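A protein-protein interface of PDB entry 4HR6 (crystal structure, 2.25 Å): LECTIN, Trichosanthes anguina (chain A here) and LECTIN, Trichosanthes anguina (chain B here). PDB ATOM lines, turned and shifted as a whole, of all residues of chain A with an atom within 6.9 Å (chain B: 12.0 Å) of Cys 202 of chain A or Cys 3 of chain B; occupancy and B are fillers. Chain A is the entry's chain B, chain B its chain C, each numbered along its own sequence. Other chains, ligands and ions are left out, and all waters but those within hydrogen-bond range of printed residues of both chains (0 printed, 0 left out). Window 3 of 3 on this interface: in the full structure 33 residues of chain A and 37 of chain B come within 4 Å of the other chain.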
ATOM      1  N   LEU A 155      18.787  -5.085  18.723  1.00  0.00           N
ATOM      2  CA  LEU A 155      18.496  -5.980  19.849  1.00  0.00           C
ATOM      3  C   LEU A 155      17.282  -5.491  20.636  1.00  0.00           C
ATOM      4  O   LEU A 155      16.416  -6.278  20.982  1.00  0.00           O
ATOM      5  CB  LEU A 155      19.691  -6.073  20.816  1.00  0.00           C
ATOM      6  CG  LEU A 155      19.468  -6.879  22.108  1.00  0.00           C
ATOM      7  CD1 LEU A 155      19.173  -8.333  21.830  1.00  0.00           C
ATOM      8  CD2 LEU A 155      20.690  -6.813  22.992  1.00  0.00           C
ATOM      9  N   GLN A 158      13.901  -6.094  18.932  1.00  0.00           N
ATOM     10  CA  GLN A 158      13.482  -7.486  19.087  1.00  0.00           C
ATOM     11  C   GLN A 158      13.030  -7.788  20.510  1.00  0.00           C
ATOM     12  O   GLN A 158      11.999  -8.433  20.730  1.00  0.00           O
ATOM     13  CB  GLN A 158      14.573  -8.436  18.627  1.00  0.00           C
ATOM     14  CG  GLN A 158      14.707  -8.453  17.098  1.00  0.00           C
ATOM     15  CD  GLN A 158      16.103  -8.803  16.596  1.00  0.00           C
ATOM     16  OE1 GLN A 158      16.682  -9.822  16.977  1.00  0.00           O
ATOM     17  NE2 GLN A 158      16.637  -7.968  15.715  1.00  0.00           N
ATOM     18  N   ALA A 159      13.775  -7.268  21.469  1.00  0.00           N
ATOM     19  CA  ALA A 159      13.485  -7.468  22.861  1.00  0.00           C
ATOM     20  C   ALA A 159      12.143  -6.848  23.256  1.00  0.00           C
ATOM     21  O   ALA A 159      11.413  -7.402  24.080  1.00  0.00           O
ATOM     22  CB  ALA A 159      14.600  -6.874  23.688  1.00  0.00           C
ATOM     23  N   SER A 160      11.825  -5.704  22.650  1.00  0.00           N
ATOM     24  CA  SER A 160      10.604  -4.960  22.944  1.00  0.00           C
ATOM     25  C   SER A 160       9.324  -5.724  22.656  1.00  0.00           C
ATOM     26  O   SER A 160       8.273  -5.372  23.180  1.00  0.00           O
ATOM     27  CB  SER A 160      10.567  -3.665  22.138  1.00  0.00           C
ATOM     28  OG  SER A 160      10.135  -3.935  20.805  1.00  0.00           O
ATOM     29  N   THR A 161       9.396  -6.760  21.828  1.00  0.00           N
ATOM     30  CA  THR A 161       8.209  -7.527  21.508  1.00  0.00           C
ATOM     31  C   THR A 161       7.665  -8.308  22.701  1.00  0.00           C
ATOM     32  O   THR A 161       6.520  -8.752  22.659  1.00  0.00           O
ATOM     33  CB  THR A 161       8.457  -8.543  20.392  1.00  0.00           C
ATOM     34  OG1 THR A 161       9.501  -9.434  20.783  1.00  0.00           O
ATOM     35  CG2 THR A 161       8.832  -7.837  19.099  1.00  0.00           C
ATOM     36  N   SER A 162       8.487  -8.505  23.739  1.00  0.00           N
ATOM     37  CA  SER A 162       8.060  -9.238  24.944  1.00  0.00           C
ATOM     38  C   SER A 162       7.401  -8.333  25.988  1.00  0.00           C
ATOM     39  O   SER A 162       6.811  -8.824  26.922  1.00  0.00           O
ATOM     40  CB  SER A 162       9.247  -9.969  25.593  1.00  0.00           C
ATOM     41  OG  SER A 162      10.187  -9.046  26.121  1.00  0.00           O
ATOM     42  N   LEU A 199      19.739  -5.863  12.476  1.00  0.00           N
ATOM     43  CA  LEU A 199      20.542  -7.053  12.729  1.00  0.00           C
ATOM     44  C   LEU A 199      19.730  -8.087  13.508  1.00  0.00           C
ATOM     45  O   LEU A 199      19.093  -7.754  14.509  1.00  0.00           O
ATOM     46  CB  LEU A 199      21.783  -6.666  13.535  1.00  0.00           C
ATOM     47  CG  LEU A 199      22.844  -7.739  13.797  1.00  0.00           C
ATOM     48  CD1 LEU A 199      23.550  -8.152  12.520  1.00  0.00           C
ATOM     49  CD2 LEU A 199      23.845  -7.188  14.797  1.00  0.00           C
ATOM     50  N   TYR A 200      19.770  -9.332  13.049  1.00  0.00           N
ATOM     51  CA  TYR A 200      19.188 -10.457  13.778  1.00  0.00           C
ATOM     52  C   TYR A 200      19.927 -10.781  15.089  1.00  0.00           C
ATOM     53  O   TYR A 200      21.131 -10.950  15.110  1.00  0.00           O
ATOM     54  CB  TYR A 200      19.182 -11.700  12.892  1.00  0.00           C
ATOM     55  CG  TYR A 200      18.657 -12.920  13.592  1.00  0.00           C
ATOM     56  CD1 TYR A 200      19.533 -13.831  14.187  1.00  0.00           C
ATOM     57  CD2 TYR A 200      17.292 -13.158  13.687  1.00  0.00           C
ATOM     58  CE1 TYR A 200      19.067 -14.945  14.838  1.00  0.00           C
ATOM     59  CE2 TYR A 200      16.819 -14.279  14.327  1.00  0.00           C
ATOM     60  CZ  TYR A 200      17.716 -15.167  14.910  1.00  0.00           C
ATOM     61  OH  TYR A 200      17.260 -16.285  15.550  1.00  0.00           O
ATOM     62  N   HIS A 201      19.189 -10.845  16.184  1.00  0.00           N
ATOM     63  CA  HIS A 201      19.734 -11.319  17.466  1.00  0.00           C
ATOM     64  C   HIS A 201      18.937 -12.507  17.955  1.00  0.00           C
ATOM     65  O   HIS A 201      19.526 -13.480  18.429  1.00  0.00           O
ATOM     66  CB  HIS A 201      19.667 -10.245  18.547  1.00  0.00           C
ATOM     67  CG  HIS A 201      20.654  -9.136  18.381  1.00  0.00           C
ATOM     68  ND1 HIS A 201      21.935  -9.210  18.866  1.00  0.00           N
ATOM     69  CD2 HIS A 201      20.538  -7.915  17.811  1.00  0.00           C
ATOM     70  CE1 HIS A 201      22.573  -8.082  18.602  1.00  0.00           C
ATOM     71  NE2 HIS A 201      21.743  -7.276  17.971  1.00  0.00           N
ATOM     72  N   CYS A 202      17.602 -12.425  17.875  1.00  0.00           N
ATOM     73  CA  CYS A 202      16.740 -13.453  18.452  1.00  0.00           C
ATOM     74  C   CYS A 202      15.515 -13.749  17.609  1.00  0.00           C
ATOM     75  O   CYS A 202      15.051 -12.874  16.876  1.00  0.00           O
ATOM     76  CB  CYS A 202      16.289 -13.012  19.826  1.00  0.00           C
ATOM     77  SG  CYS A 202      17.587 -13.048  21.085  1.00  0.00           S
ATOM     78  N   GLN A 203      15.006 -14.984  17.712  1.00  0.00           N
ATOM     79  CA  GLN A 203      13.799 -15.382  17.016  1.00  0.00           C
ATOM     80  C   GLN A 203      12.547 -15.068  17.827  1.00  0.00           C
ATOM     81  O   GLN A 203      12.055 -15.924  18.563  1.00  0.00           O
ATOM     82  CB  GLN A 203      13.823 -16.874  16.643  1.00  0.00           C
ATOM     83  CG  GLN A 203      13.982 -17.144  15.150  1.00  0.00           C
ATOM     84  CD  GLN A 203      12.723 -17.640  14.449  1.00  0.00           C
ATOM     85  OE1 GLN A 203      12.024 -18.529  14.941  1.00  0.00           O
ATOM     86  NE2 GLN A 203      12.458 -17.098  13.259  1.00  0.00           N
ATOM     87  N   VAL A 204      12.019 -13.855  17.670  1.00  0.00           N
ATOM     88  CA  VAL A 204      10.763 -13.451  18.352  1.00  0.00           C
ATOM     89  C   VAL A 204       9.696 -13.118  17.302  1.00  0.00           C
ATOM     90  O   VAL A 204       9.921 -13.357  16.117  1.00  0.00           O
ATOM     91  CB  VAL A 204      10.967 -12.250  19.322  1.00  0.00           C
ATOM     92  CG1 VAL A 204       9.976 -12.333  20.488  1.00  0.00           C
ATOM     93  CG2 VAL A 204      12.380 -12.225  19.891  1.00  0.00           C
ATOM     94  N   SER A 205       8.545 -12.580  17.709  1.00  0.00           N
ATOM     95  CA  SER A 205       7.537 -12.112  16.736  1.00  0.00           C
ATOM     96  C   SER A 205       6.494 -11.125  17.279  1.00  0.00           C
ATOM     97  O   SER A 205       6.168 -11.145  18.469  1.00  0.00           O
ATOM     98  CB  SER A 205       6.787 -13.308  16.140  1.00  0.00           C
ATOM     99  OG  SER A 205       5.959 -12.894  15.068  1.00  0.00           O
ATOM    100  N   ASN B   1      21.787  -7.287  28.642  1.00  0.00           N
ATOM    101  CA  ASN B   1      21.296  -7.432  27.242  1.00  0.00           C
ATOM    102  C   ASN B   1      20.707  -8.802  26.987  1.00  0.00           C
ATOM    103  O   ASN B   1      21.418  -9.793  27.040  1.00  0.00           O
ATOM    104  CB  ASN B   1      22.419  -7.189  26.241  1.00  0.00           C
ATOM    105  CG  ASN B   1      22.452  -5.766  25.735  1.00  0.00           C
ATOM    106  OD1 ASN B   1      21.705  -4.899  26.188  1.00  0.00           O
ATOM    107  ND2 ASN B   1      23.328  -5.519  24.781  1.00  0.00           N
ATOM    108  N   GLU B   2      19.409  -8.845  26.696  1.00  0.00           N
ATOM    109  CA  GLU B   2      18.734 -10.094  26.408  1.00  0.00           C
ATOM    110  C   GLU B   2      17.423  -9.763  25.686  1.00  0.00           C
ATOM    111  O   GLU B   2      16.963  -8.612  25.660  1.00  0.00           O
ATOM    112  CB  GLU B   2      18.597 -10.908  27.702  1.00  0.00           C
ATOM    113  CG  GLU B   2      17.459 -11.869  27.866  1.00  0.00           C
ATOM    114  CD  GLU B   2      17.866 -13.297  27.535  1.00  0.00           C
ATOM    115  OE1 GLU B   2      18.307 -13.947  28.537  1.00  0.00           O
ATOM    116  OE2 GLU B   2      17.709 -13.752  26.325  1.00  0.00           O
ATOM    117  N   CYS B   3      16.875 -10.792  25.066  1.00  0.00           N
ATOM    118  CA  CYS B   3      15.752 -10.690  24.191  1.00  0.00           C
ATOM    119  C   CYS B   3      14.441 -10.757  24.924  1.00  0.00           C
ATOM    120  O   CYS B   3      13.385 -10.663  24.315  1.00  0.00           O
ATOM    121  CB  CYS B   3      15.864 -11.775  23.127  1.00  0.00           C
ATOM    122  SG  CYS B   3      17.241 -11.361  22.016  1.00  0.00           S
ATOM    123  N   ILE B   4      14.511 -10.888  26.240  1.00  0.00           N
ATOM    124  CA  ILE B   4      13.321 -10.896  27.054  1.00  0.00           C
ATOM    125  C   ILE B   4      13.416  -9.798  28.092  1.00  0.00           C
ATOM    126  O   ILE B   4      14.458  -9.593  28.694  1.00  0.00           O
ATOM    127  CB  ILE B   4      13.064 -12.278  27.654  1.00  0.00           C
ATOM    128  CG1 ILE B   4      12.802 -13.260  26.506  1.00  0.00           C
ATOM    129  CG2 ILE B   4      11.858 -12.226  28.584  1.00  0.00           C
ATOM    130  CD1 ILE B   4      12.761 -14.706  26.924  1.00  0.00           C
ATOM    131  N   VAL B   5      12.332  -9.042  28.234  1.00  0.00           N
ATOM    132  CA  VAL B   5      12.277  -7.946  29.193  1.00  0.00           C
ATOM    133  C   VAL B   5      11.145  -8.267  30.151  1.00  0.00           C
ATOM    134  O   VAL B   5      10.001  -8.432  29.724  1.00  0.00           O
ATOM    135  CB  VAL B   5      11.991  -6.606  28.493  1.00  0.00           C
ATOM    136  CG1 VAL B   5      12.268  -5.459  29.437  1.00  0.00           C
ATOM    137  CG2 VAL B   5      12.834  -6.473  27.237  1.00  0.00           C
ATOM    138  N   GLU B   6      11.464  -8.384  31.431  1.00  0.00           N
ATOM    139  CA  GLU B   6      10.484  -8.855  32.418  1.00  0.00           C
ATOM    140  C   GLU B   6       9.585  -7.715  32.899  1.00  0.00           C
ATOM    141  O   GLU B   6       8.354  -7.858  32.942  1.00  0.00           O
ATOM    142  CB  GLU B   6      11.202  -9.528  33.606  1.00  0.00           C
ATOM    143  N   THR B   7      10.208  -6.598  33.276  1.00  0.00           N
ATOM    144  CA  THR B   7       9.482  -5.413  33.697  1.00  0.00           C
ATOM    145  C   THR B   7      10.271  -4.157  33.344  1.00  0.00           C
ATOM    146  O   THR B   7      11.494  -4.197  33.232  1.00  0.00           O
ATOM    147  CB  THR B   7       9.242  -5.382  35.226  1.00  0.00           C
ATOM    148  OG1 THR B   7      10.477  -5.105  35.888  1.00  0.00           O
ATOM    149  CG2 THR B   7       8.674  -6.702  35.751  1.00  0.00           C
ATOM    150  N   ARG B   8       9.567  -3.038  33.201  1.00  0.00           N
ATOM    151  CA  ARG B   8      10.207  -1.744  32.929  1.00  0.00           C
ATOM    152  C   ARG B   8       9.443  -0.610  33.588  1.00  0.00           C
ATOM    153  O   ARG B   8       8.217  -0.655  33.681  1.00  0.00           O
ATOM    154  CB  ARG B   8      10.264  -1.478  31.421  1.00  0.00           C
ATOM    155  CG  ARG B   8      11.492  -2.031  30.709  1.00  0.00           C
ATOM    156  CD  ARG B   8      12.773  -1.319  31.092  1.00  0.00           C
ATOM    157  NE  ARG B   8      12.640   0.122  31.273  1.00  0.00           N
ATOM    158  CZ  ARG B   8      12.386   1.012  30.303  1.00  0.00           C
ATOM    159  NH1 ARG B   8      12.163   0.624  29.047  1.00  0.00           N
ATOM    160  NH2 ARG B   8      12.315   2.304  30.603  1.00  0.00           N
ATOM    161  N   SER B  50       4.995  -8.386  32.888  1.00  0.00           N
ATOM    162  CA  SER B  50       4.601  -9.470  31.974  1.00  0.00           C
ATOM    163  C   SER B  50       3.131  -9.923  32.144  1.00  0.00           C
ATOM    164  O   SER B  50       2.600 -10.648  31.299  1.00  0.00           O
ATOM    165  CB  SER B  50       5.541 -10.667  32.145  1.00  0.00           C
ATOM    166  OG  SER B  50       6.889 -10.235  32.218  1.00  0.00           O
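The side-chain sulfur of Cys 3 of chain B is disulfide-bonded to the side-chain sulfur of Cys 202 of chain A. OG of Ser 162 of chain A sits at hydrogen-bond distance from N of Val 5 of chain B, 3.0 Å away.
The backbone carbonyl oxygen (O) of Ala 159 of chain A is in hydrogen-bond range of the side-chain hydroxyl (OG) of Ser 162 of chain A (2.9 Å). The side-chain amide oxygen of Gln 158 of chain A lies within hydrogen-bond range of the backbone NH of Cys 202 of chain A, 2.9 Å away.
Among the printed residues, merely in contact across the chains: Leu 155 of chain A with Asn 1 of chain B (3.4 Å), Leu 155 of chain A with Cys 3 of chain B (3.6 Å), Ala 159 of chain A with Glu 2 of chain B (3.5 Å), Ala 159 of chain A with Cys 3 of chain B (3.5 Å), Ala 159 of chain A with Val 5 of chain B (3.6 Å) and Ser 162 of chain A with Ile 4 of chain B (3.8 Å).
No residue of chain B comes within 4 Å of Gln 158 of chain A. No residue of chain B comes within 4 Å of Thr 161 of chain A. Of the printed residues of chain B, Ser 162 of chain A touches Ile 4 and Val 5. Leu 199 of chain A touches none of the printed residues of chain B. Tyr 200 of chain A touches none of the printed residues of chain B. Cys 202 of chain A touches one residue of chain B. No residue of chain B comes within 4 Å of Val 204 of chain A. Printed residues of chain A within 4 Å of Glu 2 of chain B: Ala 159 (3.5 Å). Of the printed residues of chain A, Cys 3 of chain B touches Leu 155 (3.6 Å), Ala 159 (3.5 Å) and Cys 202 (2.0 Å). Of the printed residues of chain A, Ile 4 of chain B touches Ser 162. Of the printed residues of chain A, Val 5 of chain B touches Ala 159 (3.6 Å) and Ser 162 (3.0 Å). Thr 7 of chain B touches none of the printed residues of chain A. The nearest printed residue of chain A that does not touch Cys 3 of chain B is Ser 162 of chain A (4.01 Å).
Printed residues of chain B that touch a printed residue of chain A: Asn 1, Glu 2, Cys 3, Ile 4 and Val 5. Hydrophobic or aromatic side chains of chain B that line the printed part of chain A: Val 5. Of the 13 printed residues of chain A, 4 touch a printed residue of chain B. Along chain A the printed residues that touch a printed residue of chain B span positions 155 to 202. Among the printed residues, 8 pairs touch across the chains. Among the printed residues, no Asp or Glu carboxylate lies within 4 Å of a Lys or Arg side-chain nitrogen of the other chain.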
